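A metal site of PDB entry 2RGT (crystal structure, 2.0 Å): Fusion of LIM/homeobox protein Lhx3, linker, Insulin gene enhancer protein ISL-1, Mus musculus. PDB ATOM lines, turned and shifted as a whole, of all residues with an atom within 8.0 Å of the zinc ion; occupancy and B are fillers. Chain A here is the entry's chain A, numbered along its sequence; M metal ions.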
ATOM      1  N   LYS A  67     -19.898 -18.808  11.072  1.00  0.00           N
ATOM      2  CA  LYS A  67     -19.968 -20.101  11.710  1.00  0.00           C
ATOM      3  C   LYS A  67     -21.181 -20.192  12.611  1.00  0.00           C
ATOM      4  O   LYS A  67     -21.503 -19.259  13.299  1.00  0.00           O
ATOM      5  CB  LYS A  67     -18.694 -20.301  12.552  1.00  0.00           C
ATOM      6  CG  LYS A  67     -17.381 -20.505  11.800  1.00  0.00           C
ATOM      7  CD  LYS A  67     -17.453 -21.423  10.605  1.00  0.00           C
ATOM      8  CE  LYS A  67     -16.066 -21.720  10.066  1.00  0.00           C
ATOM      9  NZ  LYS A  67     -15.607 -20.650   9.119  1.00  0.00           N
ATOM     10  N   CYS A  68     -21.873 -21.344  12.653  1.00  0.00           N
ATOM     11  CA  CYS A  68     -22.835 -21.549  13.725  1.00  0.00           C
ATOM     12  C   CYS A  68     -22.149 -21.482  15.103  1.00  0.00           C
ATOM     13  O   CYS A  68     -21.193 -22.197  15.343  1.00  0.00           O
ATOM     14  CB  CYS A  68     -23.601 -22.845  13.500  1.00  0.00           C
ATOM     15  SG  CYS A  68     -24.604 -23.276  14.895  1.00  0.00           S
ATOM     16  N   ALA A  69     -22.614 -20.587  15.990  1.00  0.00           N
ATOM     17  CA  ALA A  69     -22.060 -20.473  17.346  1.00  0.00           C
ATOM     18  C   ALA A  69     -22.087 -21.708  18.224  1.00  0.00           C
ATOM     19  O   ALA A  69     -21.226 -21.873  19.086  1.00  0.00           O
ATOM     20  CB  ALA A  69     -22.710 -19.296  18.104  1.00  0.00           C
ATOM     21  N   ALA A  70     -23.083 -22.566  18.004  1.00  0.00           N
ATOM     22  CA  ALA A  70     -23.215 -23.855  18.621  1.00  0.00           C
ATOM     23  C   ALA A  70     -22.263 -24.884  18.003  1.00  0.00           C
ATOM     24  O   ALA A  70     -21.294 -25.257  18.624  1.00  0.00           O
ATOM     25  CB  ALA A  70     -24.691 -24.343  18.504  1.00  0.00           C
ATOM     26  N   CYS A  71     -22.504 -25.301  16.778  1.00  0.00           N
ATOM     27  CA  CYS A  71     -21.717 -26.387  16.180  1.00  0.00           C
ATOM     28  C   CYS A  71     -20.438 -25.933  15.412  1.00  0.00           C
ATOM     29  O   CYS A  71     -19.607 -26.764  15.009  1.00  0.00           O
ATOM     30  CB  CYS A  71     -22.608 -27.254  15.288  1.00  0.00           C
ATOM     31  SG  CYS A  71     -23.020 -26.461  13.650  1.00  0.00           S
ATOM     32  N   GLN A  72     -20.268 -24.625  15.243  1.00  0.00           N
ATOM     33  CA  GLN A  72     -19.075 -24.041  14.592  1.00  0.00           C
ATOM     34  C   GLN A  72     -18.905 -24.341  13.073  1.00  0.00           C
ATOM     35  O   GLN A  72     -17.854 -24.062  12.549  1.00  0.00           O
ATOM     36  CB  GLN A  72     -17.787 -24.388  15.355  1.00  0.00           C
ATOM     37  CG  GLN A  72     -17.541 -23.682  16.718  1.00  0.00           C
ATOM     38  CD  GLN A  72     -17.639 -22.163  16.637  1.00  0.00           C
ATOM     39  OE1 GLN A  72     -17.986 -21.488  17.629  1.00  0.00           O
ATOM     40  NE2 GLN A  72     -17.359 -21.614  15.461  1.00  0.00           N
ATOM     41  N   LEU A  73     -19.911 -24.881  12.392  1.00  0.00           N
ATOM     42  CA  LEU A  73     -19.856 -25.116  10.938  1.00  0.00           C
ATOM     43  C   LEU A  73     -20.330 -23.903  10.157  1.00  0.00           C
ATOM     44  O   LEU A  73     -21.095 -23.113  10.687  1.00  0.00           O
ATOM     45  CB  LEU A  73     -20.730 -26.289  10.499  1.00  0.00           C
ATOM     46  CG  LEU A  73     -20.533 -27.656  11.156  1.00  0.00           C
ATOM     47  CD1 LEU A  73     -21.339 -28.633  10.431  1.00  0.00           C
ATOM     48  CD2 LEU A  73     -19.089 -28.021  11.108  1.00  0.00           C
ATOM     49  N   GLY A  74     -19.864 -23.779   8.899  1.00  0.00           N
ATOM     50  CA  GLY A  74     -19.934 -22.545   8.117  1.00  0.00           C
ATOM     51  C   GLY A  74     -21.346 -22.531   7.612  1.00  0.00           C
ATOM     52  O   GLY A  74     -21.876 -23.590   7.242  1.00  0.00           O
ATOM     53  N   ILE A  75     -21.967 -21.358   7.633  1.00  0.00           N
ATOM     54  CA  ILE A  75     -23.357 -21.199   7.166  1.00  0.00           C
ATOM     55  C   ILE A  75     -23.290 -20.406   5.834  1.00  0.00           C
ATOM     56  O   ILE A  75     -22.753 -19.293   5.821  1.00  0.00           O
ATOM     57  CB  ILE A  75     -24.201 -20.429   8.178  1.00  0.00           C
ATOM     58  CG1 ILE A  75     -24.175 -21.124   9.556  1.00  0.00           C
ATOM     59  CG2 ILE A  75     -25.626 -20.217   7.630  1.00  0.00           C
ATOM     60  CD1 ILE A  75     -24.835 -20.312  10.685  1.00  0.00           C
ATOM     61  N   GLN A  79     -28.862 -20.242   3.733  1.00  0.00           N
ATOM     62  CA  GLN A  79     -29.559 -20.976   4.781  1.00  0.00           C
ATOM     63  C   GLN A  79     -30.220 -20.012   5.795  1.00  0.00           C
ATOM     64  O   GLN A  79     -29.645 -18.998   6.179  1.00  0.00           O
ATOM     65  CB  GLN A  79     -28.587 -21.880   5.479  1.00  0.00           C
ATOM     66  CG  GLN A  79     -29.233 -23.049   6.166  1.00  0.00           C
ATOM     67  CD  GLN A  79     -28.210 -23.963   6.724  1.00  0.00           C
ATOM     68  OE1 GLN A  79     -27.058 -23.581   6.830  1.00  0.00           O
ATOM     69  NE2 GLN A  79     -28.614 -25.225   7.048  1.00  0.00           N
ATOM     70  N   VAL A  81     -31.500 -19.021   9.448  1.00  0.00           N
ATOM     71  CA  VAL A  81     -30.811 -19.152  10.745  1.00  0.00           C
ATOM     72  C   VAL A  81     -31.610 -18.388  11.803  1.00  0.00           C
ATOM     73  O   VAL A  81     -32.572 -17.644  11.488  1.00  0.00           O
ATOM     74  CB  VAL A  81     -29.311 -18.674  10.727  1.00  0.00           C
ATOM     75  CG1 VAL A  81     -28.368 -19.623   9.935  1.00  0.00           C
ATOM     76  CG2 VAL A  81     -29.164 -17.234  10.220  1.00  0.00           C
ATOM     77  N   VAL A  88     -24.986 -16.314  15.484  1.00  0.00           N
ATOM     78  CA  VAL A  88     -25.939 -16.896  14.533  1.00  0.00           C
ATOM     79  C   VAL A  88     -26.014 -18.408  14.796  1.00  0.00           C
ATOM     80  O   VAL A  88     -25.049 -18.972  15.227  1.00  0.00           O
ATOM     81  CB  VAL A  88     -25.490 -16.508  13.085  1.00  0.00           C
ATOM     82  CG1 VAL A  88     -26.076 -17.351  12.119  1.00  0.00           C
ATOM     83  CG2 VAL A  88     -25.887 -15.096  12.828  1.00  0.00           C
ATOM     84  N   TYR A  89     -27.181 -19.048  14.605  1.00  0.00           N
ATOM     85  CA  TYR A  89     -27.346 -20.444  14.932  1.00  0.00           C
ATOM     86  C   TYR A  89     -28.170 -21.145  13.863  1.00  0.00           C
ATOM     87  O   TYR A  89     -29.169 -20.635  13.421  1.00  0.00           O
ATOM     88  CB  TYR A  89     -28.177 -20.609  16.254  1.00  0.00           C
ATOM     89  CG  TYR A  89     -27.530 -19.958  17.429  1.00  0.00           C
ATOM     90  CD1 TYR A  89     -26.664 -20.690  18.245  1.00  0.00           C
ATOM     91  CD2 TYR A  89     -27.739 -18.616  17.707  1.00  0.00           C
ATOM     92  CE1 TYR A  89     -26.035 -20.091  19.340  1.00  0.00           C
ATOM     93  CE2 TYR A  89     -27.080 -17.999  18.771  1.00  0.00           C
ATOM     94  CZ  TYR A  89     -26.246 -18.750  19.572  1.00  0.00           C
ATOM     95  OH  TYR A  89     -25.626 -18.163  20.628  1.00  0.00           O
ATOM     96  N   HIS A  90     -27.793 -22.371  13.526  1.00  0.00           N
ATOM     97  CA  HIS A  90     -28.649 -23.212  12.732  1.00  0.00           C
ATOM     98  C   HIS A  90     -30.038 -23.433  13.321  1.00  0.00           C
ATOM     99  O   HIS A  90     -30.194 -23.552  14.540  1.00  0.00           O
ATOM    100  CB  HIS A  90     -27.969 -24.569  12.616  1.00  0.00           C
ATOM    101  CG  HIS A  90     -26.829 -24.611  11.636  1.00  0.00           C
ATOM    102  ND1 HIS A  90     -25.544 -24.944  12.019  1.00  0.00           N
ATOM    103  CD2 HIS A  90     -26.774 -24.377  10.312  1.00  0.00           C
ATOM    104  CE1 HIS A  90     -24.747 -24.948  10.970  1.00  0.00           C
ATOM    105  NE2 HIS A  90     -25.470 -24.609   9.924  1.00  0.00           N
ATOM    106  N   LEU A  91     -31.078 -23.612  12.482  1.00  0.00           N
ATOM    107  CA  LEU A  91     -32.403 -23.913  13.052  1.00  0.00           C
ATOM    108  C   LEU A  91     -32.340 -24.987  14.124  1.00  0.00           C
ATOM    109  O   LEU A  91     -32.814 -24.757  15.248  1.00  0.00           O
ATOM    110  CB  LEU A  91     -33.485 -24.278  12.009  1.00  0.00           C
ATOM    111  CG  LEU A  91     -33.760 -23.125  11.048  1.00  0.00           C
ATOM    112  CD1 LEU A  91     -34.737 -23.674  10.039  1.00  0.00           C
ATOM    113  CD2 LEU A  91     -34.282 -21.845  11.804  1.00  0.00           C
ATOM    114  N   HIS A  92     -31.724 -26.104  13.768  1.00  0.00           N
ATOM    115  CA  HIS A  92     -31.538 -27.290  14.612  1.00  0.00           C
ATOM    116  C   HIS A  92     -30.567 -27.138  15.735  1.00  0.00           C
ATOM    117  O   HIS A  92     -30.530 -28.028  16.588  1.00  0.00           O
ATOM    118  CB  HIS A  92     -31.167 -28.520  13.738  1.00  0.00           C
ATOM    119  CG  HIS A  92     -29.796 -28.407  13.084  1.00  0.00           C
ATOM    120  ND1 HIS A  92     -29.570 -27.708  11.927  1.00  0.00           N
ATOM    121  CD2 HIS A  92     -28.599 -28.935  13.437  1.00  0.00           C
ATOM    122  CE1 HIS A  92     -28.294 -27.771  11.608  1.00  0.00           C
ATOM    123  NE2 HIS A  92     -27.678 -28.515  12.507  1.00  0.00           N
ATOM    124  N   CYS A  93     -29.755 -26.048  15.765  1.00  0.00           N
ATOM    125  CA  CYS A  93     -28.838 -25.747  16.860  1.00  0.00           C
ATOM    126  C   CYS A  93     -29.244 -24.635  17.885  1.00  0.00           C
ATOM    127  O   CYS A  93     -28.425 -24.276  18.765  1.00  0.00           O
ATOM    128  CB  CYS A  93     -27.482 -25.271  16.296  1.00  0.00           C
ATOM    129  SG  CYS A  93     -26.550 -26.524  15.381  1.00  0.00           S
ATOM    130  N   PHE A  94     -30.348 -23.958  17.638  1.00  0.00           N
ATOM    131  CA  PHE A  94     -30.879 -22.894  18.477  1.00  0.00           C
ATOM    132  C   PHE A  94     -31.819 -23.660  19.470  1.00  0.00           C
ATOM    133  O   PHE A  94     -33.049 -23.787  19.305  1.00  0.00           O
ATOM    134  CB  PHE A  94     -31.563 -21.849  17.553  1.00  0.00           C
ATOM    135  CG  PHE A  94     -31.995 -20.573  18.257  1.00  0.00           C
ATOM    136  CD1 PHE A  94     -31.087 -19.598  18.587  1.00  0.00           C
ATOM    137  CD2 PHE A  94     -33.332 -20.376  18.564  1.00  0.00           C
ATOM    138  CE1 PHE A  94     -31.523 -18.449  19.226  1.00  0.00           C
ATOM    139  CE2 PHE A  94     -33.794 -19.257  19.191  1.00  0.00           C
ATOM    140  CZ  PHE A  94     -32.874 -18.273  19.501  1.00  0.00           C
HETATM  141 ZN    ZN M   1     -25.079 -25.388  14.126  1.00  0.00          ZN
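SG of Cys 93 lies close to NE2 of His 92, at 3.7 Å. SG of Cys 68 lies close to N of Ala 70 (3.5 Å). The backbone carbonyl oxygen (O) of Leu 73 sits at hydrogen-bond distance from the backbone NH (N) of Cys 68, 2.8 Å away. The backbone NH (N) of Leu 73 sits close to the side-chain sulfur (SG) of Cys 71 (3.7 Å).
The nearest printed residue that does not touch the zinc ion is His 92 (4.4 Å).
The zinc ion is bound by ND1 of His 90. SG of Cys 93 is bound to the zinc ion (2.2 Å). SG of Cys 68 is bound to the zinc ion (2.3 Å). The zinc ion is bound by the side-chain sulfur (SG) of Cys 71, 2.4 Å away.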
